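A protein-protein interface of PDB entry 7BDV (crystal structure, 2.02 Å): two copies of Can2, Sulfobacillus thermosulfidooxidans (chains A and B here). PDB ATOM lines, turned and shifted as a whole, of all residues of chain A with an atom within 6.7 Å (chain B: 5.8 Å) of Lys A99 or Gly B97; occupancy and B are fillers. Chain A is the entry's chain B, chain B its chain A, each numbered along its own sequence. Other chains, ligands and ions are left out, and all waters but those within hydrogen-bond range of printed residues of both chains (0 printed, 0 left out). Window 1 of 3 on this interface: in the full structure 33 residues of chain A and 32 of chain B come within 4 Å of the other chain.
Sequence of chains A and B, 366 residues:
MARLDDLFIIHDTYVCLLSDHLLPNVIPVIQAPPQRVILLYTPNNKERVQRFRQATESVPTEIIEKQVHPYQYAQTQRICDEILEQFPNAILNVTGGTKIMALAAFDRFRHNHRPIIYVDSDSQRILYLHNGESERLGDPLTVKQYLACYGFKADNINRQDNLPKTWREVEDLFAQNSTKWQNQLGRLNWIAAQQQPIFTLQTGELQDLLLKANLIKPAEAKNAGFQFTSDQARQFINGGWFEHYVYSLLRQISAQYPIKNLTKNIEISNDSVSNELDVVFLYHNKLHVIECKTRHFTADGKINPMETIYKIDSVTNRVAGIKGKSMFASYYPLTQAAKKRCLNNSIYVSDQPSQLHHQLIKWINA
The side-chain amino group (NZ) of Lys A99 lies within hydrogen-bond range of the backbone carbonyl oxygen (O) of Thr B95 (2.9 Å).
The side-chain amino group (NZ) of Lys A99 lies close to the backbone carbonyl oxygen (O) of Gly B96 (3.3 Å).
The side-chain amino group (NZ) of Lys A99 sits at hydrogen-bond distance from the backbone carbonyl oxygen (O) of Gly B97 (2.7 Å).
The side-chain amino group (NZ) of Lys B99 sits close to the backbone carbonyl oxygen (O) of Gly A96 (3.4 Å).
O of Gly A97 lies within hydrogen-bond range of NZ of Lys B99, at 3.0 Å.
The backbone NH of Gly B97 sits at hydrogen-bond distance from the side-chain hydroxyl of Ser B19, 3.3 Å away.
N of Met B101 is in hydrogen-bond range of OG1 of Thr B98 (3.1 Å).
The side-chain hydroxyl (OG1) of Thr A98 is in hydrogen-bond range of the backbone carbonyl oxygen (O) of Pro A70 (2.7 Å).
The side-chain hydroxyl (OG1) of Thr A98 sits close to the backbone NH (N) of Ile A100.
OG1 of Thr A98 is in hydrogen-bond range of N of Met A101 (3.1 Å).
Among the printed residues, pairs that only touch across the chains: Lys A99 with Val B94 (3.1 Å), Tyr A71 with Tyr B118 (3.4 Å), Lys A99 with Ala B102 (3.6 Å), Ala A102 with Lys B99 (3.7 Å), Lys A99 with Thr B98 (3.8 Å), Thr A98 with Lys B99 (3.8 Å), Ile A100 with Tyr B118 (3.9 Å) and Lys A99 with Tyr B118 (3.9 Å).
Printed residues of chain B within 4 Å of Gly A96: Lys B99.
Of chain B, only Val B94, Thr B95, Gly B96, Gly B97, Thr B98, Ala B102 and Tyr B118 come within 4 Å of Lys A99.
Of the printed residues of chain B, Ile A100 touches Tyr B118.
Gly B97 touches just one residue of chain A: Lys A99 (2.7 Å).
The nearest printed residue of chain A that does not touch Lys B99 is Lys A99 (4.5 Å).
Of the 12 printed residues of chain B, 8 touch a printed residue of chain A.
Of the 12 printed residues of chain A, 7 touch a printed residue of chain B.
Printed residues of chain A that touch a printed residue of chain B: Tyr A71, Gly A96, Gly A97, Thr A98, Lys A99, Ile A100 and Ala A102.
Hydrophobic or aromatic side chains of chain A within 4 Å of the printed part of chain B: Tyr A71, Ile A100 and Ala A102.
Gly A96 touches Lys B99, and with the chains exchanged Lys A99 touches Gly B96.
Gly A97 touches Lys B99, and with the chains exchanged Lys A99 touches Gly B97.
Thr A98 touches Lys B99, and with the chains exchanged Lys A99 touches Thr B98.
Lys A99 touches Ala B102, and with the chains exchanged Ala A102 touches Lys B99.
Of the 13 pairs that touch across the chains among the printed residues, 8 have their exchanged pair printed and touching as well.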
ATOM      1  N   PRO A  70     -12.692  22.221   9.034  1.00  0.00           N
ATOM      2  CA  PRO A  70     -13.792  22.141   8.082  1.00  0.00           C
ATOM      3  C   PRO A  70     -14.364  23.496   7.624  1.00  0.00           C
ATOM      4  O   PRO A  70     -14.932  23.531   6.563  1.00  0.00           O
ATOM      5  CB  PRO A  70     -14.822  21.303   8.845  1.00  0.00           C
ATOM      6  CG  PRO A  70     -14.488  21.488  10.303  1.00  0.00           C
ATOM      7  CD  PRO A  70     -12.985  21.566  10.317  1.00  0.00           C
ATOM      8  N   TYR A  71     -14.161  24.586   8.366  1.00  0.00           N
ATOM      9  CA  TYR A  71     -14.859  25.881   8.129  1.00  0.00           C
ATOM     10  C   TYR A  71     -13.899  27.062   8.088  1.00  0.00           C
ATOM     11  O   TYR A  71     -14.322  28.166   8.439  1.00  0.00           O
ATOM     12  CB  TYR A  71     -15.938  26.082   9.192  1.00  0.00           C
ATOM     13  CG  TYR A  71     -16.977  25.003   9.167  1.00  0.00           C
ATOM     14  CD1 TYR A  71     -17.891  24.918   8.123  1.00  0.00           C
ATOM     15  CD2 TYR A  71     -17.025  24.028  10.159  1.00  0.00           C
ATOM     16  CE1 TYR A  71     -18.843  23.914   8.081  1.00  0.00           C
ATOM     17  CE2 TYR A  71     -17.943  22.998  10.095  1.00  0.00           C
ATOM     18  CZ  TYR A  71     -18.868  22.952   9.068  1.00  0.00           C
ATOM     19  OH  TYR A  71     -19.826  21.978   9.060  1.00  0.00           O
ATOM     20  N   TYR A  73     -11.674  28.822   5.251  1.00  0.00           N
ATOM     21  CA  TYR A  73     -11.393  29.002   3.803  1.00  0.00           C
ATOM     22  C   TYR A  73      -9.889  29.167   3.567  1.00  0.00           C
ATOM     23  O   TYR A  73      -9.300  28.356   2.825  1.00  0.00           O
ATOM     24  CB  TYR A  73     -12.150  30.221   3.274  1.00  0.00           C
ATOM     25  CG  TYR A  73     -12.118  30.379   1.777  1.00  0.00           C
ATOM     26  CD1 TYR A  73     -12.833  29.529   0.954  1.00  0.00           C
ATOM     27  CD2 TYR A  73     -11.430  31.422   1.186  1.00  0.00           C
ATOM     28  CE1 TYR A  73     -12.838  29.688  -0.426  1.00  0.00           C
ATOM     29  CE2 TYR A  73     -11.411  31.596  -0.189  1.00  0.00           C
ATOM     30  CZ  TYR A  73     -12.101  30.715  -1.003  1.00  0.00           C
ATOM     31  OH  TYR A  73     -12.096  30.868  -2.364  1.00  0.00           O
ATOM     32  N   GLY A  96     -15.574  15.363  -2.081  1.00  0.00           N
ATOM     33  CA  GLY A  96     -15.639  15.273  -0.614  1.00  0.00           C
ATOM     34  C   GLY A  96     -15.635  16.641   0.037  1.00  0.00           C
ATOM     35  O   GLY A  96     -15.429  17.668  -0.678  1.00  0.00           O
ATOM     36  N   GLY A  97     -15.842  16.655   1.352  1.00  0.00           N
ATOM     37  CA  GLY A  97     -15.496  17.775   2.249  1.00  0.00           C
ATOM     38  C   GLY A  97     -16.705  18.687   2.448  1.00  0.00           C
ATOM     39  O   GLY A  97     -17.769  18.446   1.817  1.00  0.00           O
ATOM     40  N   THR A  98     -16.537  19.727   3.240  1.00  0.00           N
ATOM     41  CA  THR A  98     -17.557  20.804   3.349  1.00  0.00           C
ATOM     42  C   THR A  98     -17.494  21.607   2.060  1.00  0.00           C
ATOM     43  O   THR A  98     -16.512  21.452   1.325  1.00  0.00           O
ATOM     44  CB  THR A  98     -17.316  21.658   4.589  1.00  0.00           C
ATOM     45  OG1 THR A  98     -16.019  22.240   4.456  1.00  0.00           O
ATOM     46  CG2 THR A  98     -17.417  20.855   5.868  1.00  0.00           C
ATOM     47  N   LYS A  99     -18.462  22.485   1.816  1.00  0.00           N
ATOM     48  CA  LYS A  99     -18.353  23.425   0.680  1.00  0.00           C
ATOM     49  C   LYS A  99     -17.186  24.389   0.914  1.00  0.00           C
ATOM     50  O   LYS A  99     -16.580  24.795  -0.071  1.00  0.00           O
ATOM     51  CB  LYS A  99     -19.671  24.168   0.467  1.00  0.00           C
ATOM     52  CG  LYS A  99     -20.752  23.279  -0.081  1.00  0.00           C
ATOM     53  CD  LYS A  99     -22.010  24.055  -0.321  1.00  0.00           C
ATOM     54  CE  LYS A  99     -22.990  23.258  -1.161  1.00  0.00           C
ATOM     55  NZ  LYS A  99     -23.824  22.389  -0.296  1.00  0.00           N
ATOM     56  N   ILE A 100     -16.852  24.730   2.165  1.00  0.00           N
ATOM     57  CA  ILE A 100     -15.718  25.652   2.459  1.00  0.00           C
ATOM     58  C   ILE A 100     -14.427  24.967   1.980  1.00  0.00           C
ATOM     59  O   ILE A 100     -13.670  25.542   1.212  1.00  0.00           O
ATOM     60  CB  ILE A 100     -15.712  26.046   3.947  1.00  0.00           C
ATOM     61  CG1 ILE A 100     -16.928  26.891   4.352  1.00  0.00           C
ATOM     62  CG2 ILE A 100     -14.423  26.715   4.352  1.00  0.00           C
ATOM     63  CD1 ILE A 100     -16.835  28.319   3.970  1.00  0.00           C
ATOM     64  N   MET A 101     -14.219  23.714   2.385  1.00  0.00           N
ATOM     65  CA  MET A 101     -13.042  22.950   1.990  1.00  0.00           C
ATOM     66  C   MET A 101     -12.967  22.883   0.470  1.00  0.00           C
ATOM     67  O   MET A 101     -11.944  23.179  -0.131  1.00  0.00           O
ATOM     68  CB  MET A 101     -13.093  21.544   2.613  1.00  0.00           C
ATOM     69  CG  MET A 101     -12.951  21.518   4.153  1.00  0.00           C
ATOM     70  SD  MET A 101     -13.312  19.735   4.947  1.00  0.00           S
ATOM     71  CE  MET A 101     -11.978  18.592   4.020  1.00  0.00           C
ATOM     72  N   ALA A 102     -14.083  22.495  -0.155  1.00  0.00           N
ATOM     73  CA  ALA A 102     -14.143  22.269  -1.583  1.00  0.00           C
ATOM     74  C   ALA A 102     -13.955  23.582  -2.338  1.00  0.00           C
ATOM     75  O   ALA A 102     -13.203  23.567  -3.332  1.00  0.00           O
ATOM     76  CB  ALA A 102     -15.449  21.608  -1.969  1.00  0.00           C
ATOM     77  N   LEU A 103     -14.605  24.675  -1.928  1.00  0.00           N
ATOM     78  CA  LEU A 103     -14.425  25.991  -2.622  1.00  0.00           C
ATOM     79  C   LEU A 103     -12.944  26.419  -2.559  1.00  0.00           C
ATOM     80  O   LEU A 103     -12.417  26.903  -3.577  1.00  0.00           O
ATOM     81  CB  LEU A 103     -15.319  27.047  -1.977  1.00  0.00           C
ATOM     82  CG  LEU A 103     -16.821  26.889  -2.235  1.00  0.00           C
ATOM     83  CD1 LEU A 103     -17.614  27.775  -1.295  1.00  0.00           C
ATOM     84  CD2 LEU A 103     -17.167  27.244  -3.666  1.00  0.00           C
ATOM     85  N   ALA A 104     -12.312  26.281  -1.401  1.00  0.00           N
ATOM     86  CA  ALA A 104     -10.907  26.686  -1.164  1.00  0.00           C
ATOM     87  C   ALA A 104      -9.987  25.924  -2.115  1.00  0.00           C
ATOM     88  O   ALA A 104      -9.154  26.552  -2.765  1.00  0.00           O
ATOM     89  CB  ALA A 104     -10.536  26.393   0.268  1.00  0.00           C
ATOM     90  N   LEU B  17     -29.595  28.166  -2.795  1.00  0.00           N
ATOM     91  CA  LEU B  17     -29.587  26.894  -3.565  1.00  0.00           C
ATOM     92  C   LEU B  17     -30.352  25.874  -2.737  1.00  0.00           C
ATOM     93  O   LEU B  17     -29.846  25.535  -1.657  1.00  0.00           O
ATOM     94  CB  LEU B  17     -28.131  26.444  -3.766  1.00  0.00           C
ATOM     95  CG  LEU B  17     -27.313  27.206  -4.792  1.00  0.00           C
ATOM     96  CD1 LEU B  17     -27.337  28.694  -4.532  1.00  0.00           C
ATOM     97  CD2 LEU B  17     -25.878  26.711  -4.787  1.00  0.00           C
ATOM     98  N   LEU B  18     -31.483  25.354  -3.223  1.00  0.00           N
ATOM     99  CA  LEU B  18     -32.335  24.432  -2.439  1.00  0.00           C
ATOM    100  C   LEU B  18     -31.810  22.994  -2.570  1.00  0.00           C
ATOM    101  O   LEU B  18     -31.389  22.589  -3.666  1.00  0.00           O
ATOM    102  CB  LEU B  18     -33.781  24.514  -2.924  1.00  0.00           C
ATOM    103  CG  LEU B  18     -34.442  25.880  -2.729  1.00  0.00           C
ATOM    104  CD1 LEU B  18     -35.959  25.755  -2.770  1.00  0.00           C
ATOM    105  CD2 LEU B  18     -34.025  26.531  -1.416  1.00  0.00           C
ATOM    106  N   SER B  19     -31.951  22.231  -1.500  1.00  0.00           N
ATOM    107  CA  SER B  19     -31.370  20.874  -1.353  1.00  0.00           C
ATOM    108  C   SER B  19     -32.052  20.172  -0.189  1.00  0.00           C
ATOM    109  O   SER B  19     -33.045  20.771   0.369  1.00  0.00           O
ATOM    110  CB  SER B  19     -29.865  20.982  -1.196  1.00  0.00           C
ATOM    111  OG  SER B  19     -29.501  21.714  -0.060  1.00  0.00           O
ATOM    112  N   VAL B  94     -24.341  30.320  -0.152  1.00  0.00           N
ATOM    113  CA  VAL B  94     -23.658  29.238  -0.916  1.00  0.00           C
ATOM    114  C   VAL B  94     -23.723  27.926  -0.103  1.00  0.00           C
ATOM    115  O   VAL B  94     -23.063  26.942  -0.496  1.00  0.00           O
ATOM    116  CB  VAL B  94     -22.211  29.677  -1.241  1.00  0.00           C
ATOM    117  CG1 VAL B  94     -21.312  29.674  -0.009  1.00  0.00           C
ATOM    118  CG2 VAL B  94     -21.564  28.871  -2.372  1.00  0.00           C
ATOM    119  N   THR B  95     -24.496  27.882   0.985  1.00  0.00           N
ATOM    120  CA  THR B  95     -24.540  26.724   1.939  1.00  0.00           C
ATOM    121  C   THR B  95     -25.318  25.554   1.307  1.00  0.00           C
ATOM    122  O   THR B  95     -24.967  24.395   1.511  1.00  0.00           O
ATOM    123  CB  THR B  95     -25.186  27.076   3.289  1.00  0.00           C
ATOM    124  OG1 THR B  95     -24.887  28.421   3.663  1.00  0.00           O
ATOM    125  CG2 THR B  95     -24.762  26.126   4.394  1.00  0.00           C
ATOM    126  N   GLY B  96     -26.381  25.848   0.566  1.00  0.00           N
ATOM    127  CA  GLY B  96     -27.200  24.829  -0.095  1.00  0.00           C
ATOM    128  C   GLY B  96     -26.554  24.259  -1.343  1.00  0.00           C
ATOM    129  O   GLY B  96     -25.531  24.790  -1.791  1.00  0.00           O
ATOM    130  N   GLY B  97     -27.157  23.201  -1.864  1.00  0.00           N
ATOM    131  CA  GLY B  97     -26.992  22.707  -3.242  1.00  0.00           C
ATOM    132  C   GLY B  97     -25.922  21.634  -3.311  1.00  0.00           C
ATOM    133  O   GLY B  97     -25.317  21.304  -2.263  1.00  0.00           O
ATOM    134  N   THR B  98     -25.672  21.119  -4.498  1.00  0.00           N
ATOM    135  CA  THR B  98     -24.504  20.239  -4.762  1.00  0.00           C
ATOM    136  C   THR B  98     -23.279  21.129  -4.721  1.00  0.00           C
ATOM    137  O   THR B  98     -23.424  22.358  -4.801  1.00  0.00           O
ATOM    138  CB  THR B  98     -24.643  19.510  -6.093  1.00  0.00           C
ATOM    139  OG1 THR B  98     -24.737  20.507  -7.128  1.00  0.00           O
ATOM    140  CG2 THR B  98     -25.853  18.617  -6.133  1.00  0.00           C
ATOM    141  N   LYS B  99     -22.093  20.534  -4.672  1.00  0.00           N
ATOM    142  CA  LYS B  99     -20.849  21.304  -4.872  1.00  0.00           C
ATOM    143  C   LYS B  99     -20.814  21.921  -6.279  1.00  0.00           C
ATOM    144  O   LYS B  99     -20.258  22.989  -6.392  1.00  0.00           O
ATOM    145  CB  LYS B  99     -19.636  20.430  -4.561  1.00  0.00           C
ATOM    146  CG  LYS B  99     -19.559  20.097  -3.088  1.00  0.00           C
ATOM    147  CD  LYS B  99     -18.320  19.365  -2.755  1.00  0.00           C
ATOM    148  CE  LYS B  99     -18.227  19.187  -1.265  1.00  0.00           C
ATOM    149  NZ  LYS B  99     -18.774  17.876  -0.918  1.00  0.00           N
ATOM    150  N   MET B 101     -23.397  23.115  -8.130  1.00  0.00           N
ATOM    151  CA  MET B 101     -24.257  24.296  -8.029  1.00  0.00           C
ATOM    152  C   MET B 101     -23.500  25.400  -7.296  1.00  0.00           C
ATOM    153  O   MET B 101     -23.405  26.540  -7.766  1.00  0.00           O
ATOM    154  CB  MET B 101     -25.553  23.942  -7.282  1.00  0.00           C
ATOM    155  CG  MET B 101     -26.496  23.008  -8.041  1.00  0.00           C
ATOM    156  SD  MET B 101     -27.982  22.272  -7.020  1.00  0.00           S
ATOM    157  CE  MET B 101     -28.933  23.991  -6.471  1.00  0.00           C
ATOM    158  N   ALA B 102     -22.962  25.041  -6.114  1.00  0.00           N
ATOM    159  CA  ALA B 102     -22.318  25.987  -5.239  1.00  0.00           C
ATOM    160  C   ALA B 102     -21.056  26.541  -5.893  1.00  0.00           C
ATOM    161  O   ALA B 102     -20.860  27.751  -5.786  1.00  0.00           O
ATOM    162  CB  ALA B 102     -22.009  25.359  -3.893  1.00  0.00           C
ATOM    163  N   TYR B 118     -22.078  31.803   4.257  1.00  0.00           N
ATOM    164  CA  TYR B 118     -22.125  30.349   4.495  1.00  0.00           C
ATOM    165  C   TYR B 118     -22.494  30.154   5.962  1.00  0.00           C
ATOM    166  O   TYR B 118     -21.900  30.820   6.809  1.00  0.00           O
ATOM    167  CB  TYR B 118     -20.787  29.710   4.124  1.00  0.00           C
ATOM    168  CG  TYR B 118     -20.741  28.232   4.413  1.00  0.00           C
ATOM    169  CD1 TYR B 118     -20.441  27.764   5.685  1.00  0.00           C
ATOM    170  CD2 TYR B 118     -20.998  27.299   3.418  1.00  0.00           C
ATOM    171  CE1 TYR B 118     -20.413  26.399   5.953  1.00  0.00           C
ATOM    172  CE2 TYR B 118     -20.992  25.933   3.680  1.00  0.00           C
ATOM    173  CZ  TYR B 118     -20.667  25.491   4.950  1.00  0.00           C
ATOM    174  OH  TYR B 118     -20.675  24.155   5.216  1.00  0.00           O
